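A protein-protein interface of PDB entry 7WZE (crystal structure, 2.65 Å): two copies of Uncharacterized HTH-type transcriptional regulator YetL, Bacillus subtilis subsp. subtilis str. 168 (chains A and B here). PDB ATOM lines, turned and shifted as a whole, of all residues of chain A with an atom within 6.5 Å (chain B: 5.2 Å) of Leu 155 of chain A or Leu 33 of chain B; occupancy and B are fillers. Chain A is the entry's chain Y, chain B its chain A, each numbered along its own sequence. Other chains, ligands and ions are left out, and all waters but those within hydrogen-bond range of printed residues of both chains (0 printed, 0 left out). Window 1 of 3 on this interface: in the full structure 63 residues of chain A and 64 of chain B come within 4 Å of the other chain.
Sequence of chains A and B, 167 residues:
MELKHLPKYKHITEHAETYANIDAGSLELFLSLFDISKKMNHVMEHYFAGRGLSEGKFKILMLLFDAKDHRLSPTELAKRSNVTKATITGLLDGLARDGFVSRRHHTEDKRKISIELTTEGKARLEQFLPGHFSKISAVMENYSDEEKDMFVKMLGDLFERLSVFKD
Leu 33 of chain A touches Leu 155 of chain B, and with the chains exchanged Leu 155 of chain A touches Leu 33 of chain B.
Ile 36 of chain A touches Leu 155 of chain B, and with the chains exchanged Leu 155 of chain A touches Ile 36 of chain B.
Phe 151 of chain B touches its own counterpart, Phe 151 of chain A.
Phe 151 of chain A touches Leu 158 of chain B, and with the chains exchanged Leu 158 of chain A touches Phe 151 of chain B.
Positions printed for both chains: 33, 36, 37, 151, 155 and 158.
Of the 27 pairs that touch across the chains among the printed residues, 10 have their exchanged pair printed and touching as well.
SD of Met 40 of chain A lies within hydrogen-bond range of OG of Ser 37 of chain B, 3.8 Å away.
Leu 155 of chain A touches just these residues of chain B: Leu 6, Leu 29, Leu 33 and Ile 36.
Of chain A, only Met 40 and Leu 155 come within 4 Å of Leu 33 of chain B.
Printed residues of chain A within 4 Å of Phe 151 of chain B: Phe 151, Met 154 and Leu 158.
Printed residues of chain A within 4 Å of Ser 37 of chain B: Ser 37 and Met 40.
Printed residues of chain A within 4 Å of Leu 158 of chain B: Ile 36, Met 140 and Phe 151.
Met 150 of chain A touches none of the printed residues of chain B.
The nearest residue of chain B that does not touch Leu 155 of chain A is Phe 151 of chain B (4.03 Å).
Hydrophobic or aromatic side chains of chain B within 4 Å of the printed part of chain A: Leu 6, Leu 29, Leu 33, Phe 34, Ile 36, Phe 151, Leu 155 and Leu 158.
Along chain B the printed residues that touch a printed residue of chain A span positions 6 to 158.
Printed residues of chain A that touch a printed residue of chain B: Leu 33, Ile 36, Ser 37, Met 40, Met 140, Phe 151, Val 152, Met 154, Leu 155, Gly 156, Leu 158 and Phe 159.
Hydrophobic or aromatic side chains of chain A that line the printed part of chain B: Leu 33, Ile 36, Met 40, Met 140, Phe 151, Val 152, Met 154, Leu 155, Leu 158 and Phe 159.
Among the printed residues, no Asp or Glu carboxylate lies within 4 Å of a Lys or Arg side-chain nitrogen of the other chain.
Among the printed residues, merely in contact across the chains: Phe 151 of chain A with Phe 151 of chain B (3.1 Å), Met 154 of chain A with Phe 151 of chain B (3.3 Å), Phe 151 of chain A with Leu 158 of chain B (3.3 Å), Phe 159 of chain A with Leu 6 of chain B (3.4 Å), Met 140 of chain A with Leu 158 of chain B (3.4 Å), Met 140 of chain A with Leu 29 of chain B (3.5 Å), Phe 151 of chain A with Leu 155 of chain B (3.5 Å), Ser 37 of chain A with Ser 37 of chain B (3.5 Å), Phe 151 of chain A with Leu 29 of chain B (3.6 Å), Gly 156 of chain A with Leu 6 of chain B (3.6 Å), Leu 155 of chain A with Leu 29 of chain B (3.6 Å), Ile 36 of chain A with Leu 155 of chain B (3.7 Å), Leu 155 of chain A with Ile 36 of chain B (3.7 Å), Val 152 of chain A with Glu 28 of chain B (3.7 Å), Met 40 of chain A with Phe 34 of chain B (3.7 Å), Leu 158 of chain A with Ile 36 of chain B (3.7 Å), Val 152 of chain A with Ser 32 of chain B (3.8 Å), Leu 158 of chain A with Phe 151 of chain B (3.8 Å), Leu 155 of chain A with Leu 6 of chain B (3.8 Å), Leu 33 of chain A with Leu 155 of chain B (3.8 Å), Ile 36 of chain A with Leu 158 of chain B (3.9 Å), Phe 159 of chain A with Ile 36 of chain B (3.9 Å), Phe 159 of chain A with Asp 35 of chain B (3.9 Å), Met 40 of chain A with Leu 33 of chain B (3.9 Å), Leu 33 of chain A with Ile 36 of chain B (3.96 Å) and Leu 155 of chain A with Leu 33 of chain B (3.97 Å).
The backbone carbonyl oxygen (O) of Glu 28 of chain B lies within hydrogen-bond range of the side-chain hydroxyl (OG) of Ser 32 of chain B, at 2.7 Å.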
ATOM      1  N   LEU A  33     -20.071   6.397 -10.959  1.00  0.00           N
ATOM      2  CA  LEU A  33     -20.263   5.910 -12.313  1.00  0.00           C
ATOM      3  C   LEU A  33     -21.265   4.772 -12.342  1.00  0.00           C
ATOM      4  O   LEU A  33     -22.026   4.631 -13.309  1.00  0.00           O
ATOM      5  CB  LEU A  33     -18.923   5.472 -12.901  1.00  0.00           C
ATOM      6  CG  LEU A  33     -18.951   5.350 -14.416  1.00  0.00           C
ATOM      7  CD1 LEU A  33     -19.491   6.621 -15.032  1.00  0.00           C
ATOM      8  CD2 LEU A  33     -17.544   5.046 -14.951  1.00  0.00           C
ATOM      9  N   ILE A  36     -24.915   6.390 -11.867  1.00  0.00           N
ATOM     10  CA  ILE A  36     -25.358   7.019 -13.104  1.00  0.00           C
ATOM     11  C   ILE A  36     -25.672   5.948 -14.137  1.00  0.00           C
ATOM     12  O   ILE A  36     -26.665   6.039 -14.866  1.00  0.00           O
ATOM     13  CB  ILE A  36     -24.308   8.031 -13.612  1.00  0.00           C
ATOM     14  CG1 ILE A  36     -24.898   8.955 -14.667  1.00  0.00           C
ATOM     15  CG2 ILE A  36     -23.130   7.350 -14.260  1.00  0.00           C
ATOM     16  CD1 ILE A  36     -24.165  10.264 -14.741  1.00  0.00           C
ATOM     17  N   SER A  37     -24.899   4.863 -14.137  1.00  0.00           N
ATOM     18  CA  SER A  37     -25.110   3.822 -15.130  1.00  0.00           C
ATOM     19  C   SER A  37     -26.470   3.161 -14.959  1.00  0.00           C
ATOM     20  O   SER A  37     -27.212   2.985 -15.937  1.00  0.00           O
ATOM     21  CB  SER A  37     -23.985   2.797 -15.053  1.00  0.00           C
ATOM     22  OG  SER A  37     -24.506   1.485 -15.169  1.00  0.00           O
ATOM     23  N   MET A  40     -29.235   5.672 -16.176  1.00  0.00           N
ATOM     24  CA  MET A  40     -29.329   5.895 -17.613  1.00  0.00           C
ATOM     25  C   MET A  40     -29.918   4.716 -18.365  1.00  0.00           C
ATOM     26  O   MET A  40     -30.742   4.888 -19.247  1.00  0.00           O
ATOM     27  CB  MET A  40     -27.972   6.212 -18.187  1.00  0.00           C
ATOM     28  CG  MET A  40     -28.061   6.557 -19.631  1.00  0.00           C
ATOM     29  SD  MET A  40     -26.543   7.635 -20.076  1.00  0.00           S
ATOM     30  CE  MET A  40     -26.523   8.761 -18.490  1.00  0.00           C
ATOM     31  N   MET A 140     -25.965  18.708 -21.640  1.00  0.00           N
ATOM     32  CA  MET A 140     -24.604  19.234 -21.587  1.00  0.00           C
ATOM     33  C   MET A 140     -24.572  20.735 -21.716  1.00  0.00           C
ATOM     34  O   MET A 140     -24.062  21.265 -22.703  1.00  0.00           O
ATOM     35  CB  MET A 140     -23.759  18.622 -22.695  1.00  0.00           C
ATOM     36  CG  MET A 140     -24.280  17.296 -23.170  1.00  0.00           C
ATOM     37  SD  MET A 140     -23.407  15.783 -22.315  1.00  0.00           S
ATOM     38  CE  MET A 140     -22.450  16.697 -20.888  1.00  0.00           C
ATOM     39  N   MET A 150     -11.889  16.041 -22.432  1.00  0.00           N
ATOM     40  CA  MET A 150     -11.274  15.309 -21.335  1.00  0.00           C
ATOM     41  C   MET A 150     -12.245  14.262 -20.813  1.00  0.00           C
ATOM     42  O   MET A 150     -11.855  13.135 -20.498  1.00  0.00           O
ATOM     43  CB  MET A 150     -10.863  16.244 -20.204  1.00  0.00           C
ATOM     44  CG  MET A 150     -10.240  15.508 -19.034  1.00  0.00           C
ATOM     45  SD  MET A 150     -10.603  16.358 -17.320  1.00  0.00           S
ATOM     46  CE  MET A 150      -9.391  17.883 -17.457  1.00  0.00           C
ATOM     47  N   PHE A 151     -13.520  14.647 -20.735  1.00  0.00           N
ATOM     48  CA  PHE A 151     -14.539  13.738 -20.231  1.00  0.00           C
ATOM     49  C   PHE A 151     -14.680  12.526 -21.140  1.00  0.00           C
ATOM     50  O   PHE A 151     -14.771  11.390 -20.665  1.00  0.00           O
ATOM     51  CB  PHE A 151     -15.870  14.460 -20.095  1.00  0.00           C
ATOM     52  CG  PHE A 151     -16.800  13.825 -19.108  1.00  0.00           C
ATOM     53  CD1 PHE A 151     -16.400  12.737 -18.358  1.00  0.00           C
ATOM     54  CD2 PHE A 151     -18.074  14.331 -18.905  1.00  0.00           C
ATOM     55  CE1 PHE A 151     -17.260  12.174 -17.440  1.00  0.00           C
ATOM     56  CE2 PHE A 151     -18.931  13.758 -17.975  1.00  0.00           C
ATOM     57  CZ  PHE A 151     -18.520  12.678 -17.249  1.00  0.00           C
ATOM     58  N   VAL A 152     -14.744  12.755 -22.456  1.00  0.00           N
ATOM     59  CA  VAL A 152     -14.788  11.622 -23.375  1.00  0.00           C
ATOM     60  C   VAL A 152     -13.482  10.844 -23.307  1.00  0.00           C
ATOM     61  O   VAL A 152     -13.484   9.610 -23.380  1.00  0.00           O
ATOM     62  CB  VAL A 152     -15.101  12.077 -24.814  1.00  0.00           C
ATOM     63  CG1 VAL A 152     -14.017  12.988 -25.352  1.00  0.00           C
ATOM     64  CG2 VAL A 152     -15.247  10.862 -25.718  1.00  0.00           C
ATOM     65  N   LYS A 153     -12.356  11.535 -23.114  1.00  0.00           N
ATOM     66  CA  LYS A 153     -11.080  10.835 -23.023  1.00  0.00           C
ATOM     67  C   LYS A 153     -11.102   9.844 -21.868  1.00  0.00           C
ATOM     68  O   LYS A 153     -10.890   8.645 -22.065  1.00  0.00           O
ATOM     69  CB  LYS A 153      -9.923  11.833 -22.879  1.00  0.00           C
ATOM     70  CG  LYS A 153      -8.662  11.464 -23.688  1.00  0.00           C
ATOM     71  CD  LYS A 153      -7.559  12.532 -23.583  1.00  0.00           C
ATOM     72  CE  LYS A 153      -6.311  12.176 -24.405  1.00  0.00           C
ATOM     73  NZ  LYS A 153      -5.295  13.277 -24.422  1.00  0.00           N
ATOM     74  N   MET A 154     -11.419  10.319 -20.666  1.00  0.00           N
ATOM     75  CA  MET A 154     -11.539   9.456 -19.490  1.00  0.00           C
ATOM     76  C   MET A 154     -12.514   8.292 -19.707  1.00  0.00           C
ATOM     77  O   MET A 154     -12.246   7.163 -19.304  1.00  0.00           O
ATOM     78  CB  MET A 154     -11.975  10.281 -18.270  1.00  0.00           C
ATOM     79  CG  MET A 154     -11.020  11.422 -17.893  1.00  0.00           C
ATOM     80  SD  MET A 154     -11.414  12.355 -16.197  1.00  0.00           S
ATOM     81  CE  MET A 154     -10.852  10.990 -14.915  1.00  0.00           C
ATOM     82  N   LEU A 155     -13.646   8.565 -20.358  1.00  0.00           N
ATOM     83  CA  LEU A 155     -14.609   7.501 -20.636  1.00  0.00           C
ATOM     84  C   LEU A 155     -14.005   6.404 -21.501  1.00  0.00           C
ATOM     85  O   LEU A 155     -14.411   5.241 -21.399  1.00  0.00           O
ATOM     86  CB  LEU A 155     -15.857   8.086 -21.295  1.00  0.00           C
ATOM     87  CG  LEU A 155     -16.760   8.738 -20.251  1.00  0.00           C
ATOM     88  CD1 LEU A 155     -17.794   9.642 -20.865  1.00  0.00           C
ATOM     89  CD2 LEU A 155     -17.433   7.648 -19.454  1.00  0.00           C
ATOM     90  N   GLY A 156     -13.046   6.750 -22.361  1.00  0.00           N
ATOM     91  CA  GLY A 156     -12.386   5.730 -23.159  1.00  0.00           C
ATOM     92  C   GLY A 156     -11.596   4.738 -22.321  1.00  0.00           C
ATOM     93  O   GLY A 156     -11.718   3.524 -22.495  1.00  0.00           O
ATOM     94  N   ASP A 157     -10.783   5.240 -21.388  1.00  0.00           N
ATOM     95  CA  ASP A 157      -9.970   4.330 -20.585  1.00  0.00           C
ATOM     96  C   ASP A 157     -10.839   3.471 -19.673  1.00  0.00           C
ATOM     97  O   ASP A 157     -10.599   2.264 -19.548  1.00  0.00           O
ATOM     98  CB  ASP A 157      -8.922   5.110 -19.789  1.00  0.00           C
ATOM     99  CG  ASP A 157      -7.746   5.561 -20.656  1.00  0.00           C
ATOM    100  OD1 ASP A 157      -7.927   6.474 -21.490  1.00  0.00           O
ATOM    101  OD2 ASP A 157      -6.634   5.002 -20.503  1.00  0.00           O
ATOM    102  N   LEU A 158     -11.847   4.070 -19.030  1.00  0.00           N
ATOM    103  CA  LEU A 158     -12.737   3.281 -18.180  1.00  0.00           C
ATOM    104  C   LEU A 158     -13.470   2.223 -18.980  1.00  0.00           C
ATOM    105  O   LEU A 158     -13.747   1.130 -18.467  1.00  0.00           O
ATOM    106  CB  LEU A 158     -13.750   4.159 -17.442  1.00  0.00           C
ATOM    107  CG  LEU A 158     -13.330   5.184 -16.382  1.00  0.00           C
ATOM    108  CD1 LEU A 158     -11.819   5.172 -16.133  1.00  0.00           C
ATOM    109  CD2 LEU A 158     -13.859   6.599 -16.676  1.00  0.00           C
ATOM    110  N   PHE A 159     -13.840   2.540 -20.219  1.00  0.00           N
ATOM    111  CA  PHE A 159     -14.563   1.566 -21.020  1.00  0.00           C
ATOM    112  C   PHE A 159     -13.758   0.285 -21.191  1.00  0.00           C
ATOM    113  O   PHE A 159     -14.303  -0.815 -21.062  1.00  0.00           O
ATOM    114  CB  PHE A 159     -14.946   2.157 -22.373  1.00  0.00           C
ATOM    115  CG  PHE A 159     -15.935   1.316 -23.133  1.00  0.00           C
ATOM    116  CD1 PHE A 159     -17.296   1.490 -22.962  1.00  0.00           C
ATOM    117  CD2 PHE A 159     -15.499   0.329 -24.005  1.00  0.00           C
ATOM    118  CE1 PHE A 159     -18.203   0.701 -23.662  1.00  0.00           C
ATOM    119  CE2 PHE A 159     -16.394  -0.462 -24.696  1.00  0.00           C
ATOM    120  CZ  PHE A 159     -17.745  -0.280 -24.529  1.00  0.00           C
ATOM    121  N   GLU A 160     -12.465   0.402 -21.491  1.00  0.00           N
ATOM    122  CA  GLU A 160     -11.687  -0.807 -21.710  1.00  0.00           C
ATOM    123  C   GLU A 160     -11.374  -1.512 -20.403  1.00  0.00           C
ATOM    124  O   GLU A 160     -11.377  -2.746 -20.360  1.00  0.00           O
ATOM    125  CB  GLU A 160     -10.387  -0.492 -22.462  1.00  0.00           C
ATOM    126  CG  GLU A 160      -9.213  -0.033 -21.601  1.00  0.00           C
ATOM    127  CD  GLU A 160      -7.971   0.319 -22.403  1.00  0.00           C
ATOM    128  OE1 GLU A 160      -8.088   0.515 -23.628  1.00  0.00           O
ATOM    129  OE2 GLU A 160      -6.877   0.397 -21.800  1.00  0.00           O
ATOM    130  N   LEU B   6     -14.055   1.882 -26.656  1.00  0.00           N
ATOM    131  CA  LEU B   6     -15.188   2.794 -26.717  1.00  0.00           C
ATOM    132  C   LEU B   6     -15.473   3.217 -28.165  1.00  0.00           C
ATOM    133  O   LEU B   6     -14.569   3.690 -28.847  1.00  0.00           O
ATOM    134  CB  LEU B   6     -14.913   4.013 -25.862  1.00  0.00           C
ATOM    135  CG  LEU B   6     -15.999   5.071 -25.781  1.00  0.00           C
ATOM    136  CD1 LEU B   6     -17.215   4.523 -25.074  1.00  0.00           C
ATOM    137  CD2 LEU B   6     -15.418   6.235 -25.029  1.00  0.00           C
ATOM    138  N   GLU B  28     -21.248  13.153 -28.801  1.00  0.00           N
ATOM    139  CA  GLU B  28     -20.266  12.105 -28.564  1.00  0.00           C
ATOM    140  C   GLU B  28     -20.169  11.805 -27.082  1.00  0.00           C
ATOM    141  O   GLU B  28     -20.065  10.642 -26.683  1.00  0.00           O
ATOM    142  CB  GLU B  28     -18.895  12.498 -29.105  1.00  0.00           C
ATOM    143  CG  GLU B  28     -17.981  11.289 -29.287  1.00  0.00           C
ATOM    144  CD  GLU B  28     -16.509  11.647 -29.298  1.00  0.00           C
ATOM    145  OE1 GLU B  28     -16.180  12.850 -29.233  1.00  0.00           O
ATOM    146  OE2 GLU B  28     -15.681  10.716 -29.390  1.00  0.00           O
ATOM    147  N   LEU B  29     -20.229  12.844 -26.253  1.00  0.00           N
ATOM    148  CA  LEU B  29     -20.157  12.640 -24.815  1.00  0.00           C
ATOM    149  C   LEU B  29     -21.379  11.893 -24.306  1.00  0.00           C
ATOM    150  O   LEU B  29     -21.268  11.039 -23.421  1.00  0.00           O
ATOM    151  CB  LEU B  29     -19.988  13.972 -24.102  1.00  0.00           C
ATOM    152  CG  LEU B  29     -19.971  13.889 -22.580  1.00  0.00           C
ATOM    153  CD1 LEU B  29     -19.039  12.799 -22.073  1.00  0.00           C
ATOM    154  CD2 LEU B  29     -19.520  15.234 -22.071  1.00  0.00           C
ATOM    155  N   PHE B  30     -22.552  12.205 -24.846  1.00  0.00           N
ATOM    156  CA  PHE B  30     -23.761  11.526 -24.409  1.00  0.00           C
ATOM    157  C   PHE B  30     -23.759  10.072 -24.851  1.00  0.00           C
ATOM    158  O   PHE B  30     -24.094   9.181 -24.066  1.00  0.00           O
ATOM    159  CB  PHE B  30     -24.986  12.255 -24.955  1.00  0.00           C
ATOM    160  CG  PHE B  30     -26.298  11.658 -24.526  1.00  0.00           C
ATOM    161  CD1 PHE B  30     -26.832  11.940 -23.283  1.00  0.00           C
ATOM    162  CD2 PHE B  30     -27.017  10.842 -25.394  1.00  0.00           C
ATOM    163  CE1 PHE B  30     -28.046  11.384 -22.887  1.00  0.00           C
ATOM    164  CE2 PHE B  30     -28.241  10.293 -25.011  1.00  0.00           C
ATOM    165  CZ  PHE B  30     -28.751  10.564 -23.752  1.00  0.00           C
ATOM    166  N   LEU B  31     -23.341   9.807 -26.087  1.00  0.00           N
ATOM    167  CA  LEU B  31     -23.323   8.432 -26.581  1.00  0.00           C
ATOM    168  C   LEU B  31     -22.255   7.596 -25.883  1.00  0.00           C
ATOM    169  O   LEU B  31     -22.482   6.414 -25.609  1.00  0.00           O
ATOM    170  CB  LEU B  31     -23.128   8.399 -28.096  1.00  0.00           C
ATOM    171  CG  LEU B  31     -24.337   8.550 -29.032  1.00  0.00           C
ATOM    172  CD1 LEU B  31     -25.412   7.515 -28.708  1.00  0.00           C
ATOM    173  CD2 LEU B  31     -24.920   9.922 -28.986  1.00  0.00           C
ATOM    174  N   SER B  32     -21.084   8.177 -25.594  1.00  0.00           N
ATOM    175  CA  SER B  32     -20.090   7.451 -24.806  1.00  0.00           C
ATOM    176  C   SER B  32     -20.643   7.100 -23.434  1.00  0.00           C
ATOM    177  O   SER B  32     -20.500   5.969 -22.958  1.00  0.00           O
ATOM    178  CB  SER B  32     -18.822   8.284 -24.648  1.00  0.00           C
ATOM    179  OG  SER B  32     -18.314   8.711 -25.899  1.00  0.00           O
ATOM    180  N   LEU B  33     -21.315   8.060 -22.803  1.00  0.00           N
ATOM    181  CA  LEU B  33     -21.876   7.820 -21.489  1.00  0.00           C
ATOM    182  C   LEU B  33     -22.913   6.724 -21.545  1.00  0.00           C
ATOM    183  O   LEU B  33     -23.062   5.947 -20.588  1.00  0.00           O
ATOM    184  CB  LEU B  33     -22.481   9.106 -20.959  1.00  0.00           C
ATOM    185  CG  LEU B  33     -21.631   9.716 -19.864  1.00  0.00           C
ATOM    186  CD1 LEU B  33     -22.347  10.922 -19.334  1.00  0.00           C
ATOM    187  CD2 LEU B  33     -21.447   8.673 -18.787  1.00  0.00           C
ATOM    188  N   PHE B  34     -23.613   6.620 -22.671  1.00  0.00           N
ATOM    189  CA  PHE B  34     -24.589   5.556 -22.799  1.00  0.00           C
ATOM    190  C   PHE B  34     -23.927   4.224 -23.095  1.00  0.00           C
ATOM    191  O   PHE B  34     -24.425   3.174 -22.670  1.00  0.00           O
ATOM    192  CB  PHE B  34     -25.599   5.868 -23.886  1.00  0.00           C
ATOM    193  CG  PHE B  34     -26.723   4.904 -23.898  1.00  0.00           C
ATOM    194  CD1 PHE B  34     -27.389   4.612 -22.717  1.00  0.00           C
ATOM    195  CD2 PHE B  34     -27.087   4.249 -25.050  1.00  0.00           C
ATOM    196  CE1 PHE B  34     -28.422   3.708 -22.697  1.00  0.00           C
ATOM    197  CE2 PHE B  34     -28.111   3.347 -25.020  1.00  0.00           C
ATOM    198  CZ  PHE B  34     -28.783   3.074 -23.848  1.00  0.00           C
ATOM    199  N   ASP B  35     -22.833   4.240 -23.851  1.00  0.00           N
ATOM    200  CA  ASP B  35     -22.120   2.997 -24.098  1.00  0.00           C
ATOM    201  C   ASP B  35     -21.577   2.437 -22.786  1.00  0.00           C
ATOM    202  O   ASP B  35     -21.895   1.302 -22.402  1.00  0.00           O
ATOM    203  CB  ASP B  35     -20.994   3.237 -25.103  1.00  0.00           C
ATOM    204  CG  ASP B  35     -21.494   3.339 -26.553  1.00  0.00           C
ATOM    205  OD1 ASP B  35     -22.514   2.700 -26.898  1.00  0.00           O
ATOM    206  OD2 ASP B  35     -20.850   4.052 -27.354  1.00  0.00           O
ATOM    207  N   ILE B  36     -20.841   3.265 -22.038  1.00  0.00           N
ATOM    208  CA  ILE B  36     -20.253   2.794 -20.791  1.00  0.00           C
ATOM    209  C   ILE B  36     -21.334   2.286 -19.855  1.00  0.00           C
ATOM    210  O   ILE B  36     -21.150   1.260 -19.194  1.00  0.00           O
ATOM    211  CB  ILE B  36     -19.379   3.892 -20.147  1.00  0.00           C
ATOM    212  CG1 ILE B  36     -18.535   3.294 -19.020  1.00  0.00           C
ATOM    213  CG2 ILE B  36     -20.207   5.046 -19.640  1.00  0.00           C
ATOM    214  CD1 ILE B  36     -17.240   4.040 -18.767  1.00  0.00           C
ATOM    215  N   SER B  37     -22.510   2.916 -19.865  1.00  0.00           N
ATOM    216  CA  SER B  37     -23.598   2.475 -19.001  1.00  0.00           C
ATOM    217  C   SER B  37     -24.030   1.057 -19.337  1.00  0.00           C
ATOM    218  O   SER B  37     -24.238   0.234 -18.444  1.00  0.00           O
ATOM    219  CB  SER B  37     -24.779   3.431 -19.133  1.00  0.00           C
ATOM    220  OG  SER B  37     -24.295   4.763 -19.078  1.00  0.00           O
ATOM    221  N   PHE B 151     -14.495  14.736 -12.572  1.00  0.00           N
ATOM    222  CA  PHE B 151     -15.335  13.750 -13.236  1.00  0.00           C
ATOM    223  C   PHE B 151     -16.632  13.527 -12.470  1.00  0.00           C
ATOM    224  O   PHE B 151     -17.725  13.572 -13.049  1.00  0.00           O
ATOM    225  CB  PHE B 151     -14.558  12.450 -13.367  1.00  0.00           C
ATOM    226  CG  PHE B 151     -15.098  11.494 -14.389  1.00  0.00           C
ATOM    227  CD1 PHE B 151     -14.399  11.241 -15.550  1.00  0.00           C
ATOM    228  CD2 PHE B 151     -16.274  10.804 -14.166  1.00  0.00           C
ATOM    229  CE1 PHE B 151     -14.859  10.326 -16.479  1.00  0.00           C
ATOM    230  CE2 PHE B 151     -16.745   9.887 -15.090  1.00  0.00           C
ATOM    231  CZ  PHE B 151     -16.032   9.645 -16.249  1.00  0.00           C
ATOM    232  N   LEU B 155     -20.522  14.021 -13.449  1.00  0.00           N
ATOM    233  CA  LEU B 155     -21.545  13.004 -13.203  1.00  0.00           C
ATOM    234  C   LEU B 155     -22.663  13.520 -12.301  1.00  0.00           C
ATOM    235  O   LEU B 155     -23.805  13.053 -12.392  1.00  0.00           O
ATOM    236  CB  LEU B 155     -20.921  11.764 -12.579  1.00  0.00           C
ATOM    237  CG  LEU B 155     -20.647  10.567 -13.473  1.00  0.00           C
ATOM    238  CD1 LEU B 155     -20.487  10.998 -14.886  1.00  0.00           C
ATOM    239  CD2 LEU B 155     -19.424   9.840 -12.987  1.00  0.00           C
ATOM    240  N   LEU B 158     -24.932  15.569 -14.718  1.00  0.00           N
ATOM    241  CA  LEU B 158     -25.569  14.712 -15.710  1.00  0.00           C
ATOM    242  C   LEU B 158     -26.706  13.908 -15.104  1.00  0.00           C
ATOM    243  O   LEU B 158     -27.787  13.807 -15.694  1.00  0.00           O
ATOM    244  CB  LEU B 158     -24.526  13.774 -16.314  1.00  0.00           C
ATOM    245  CG  LEU B 158     -23.425  14.510 -17.070  1.00  0.00           C
ATOM    246  CD1 LEU B 158     -22.192  13.647 -17.278  1.00  0.00           C
ATOM    247  CD2 LEU B 158     -23.998  14.956 -18.383  1.00  0.00           C
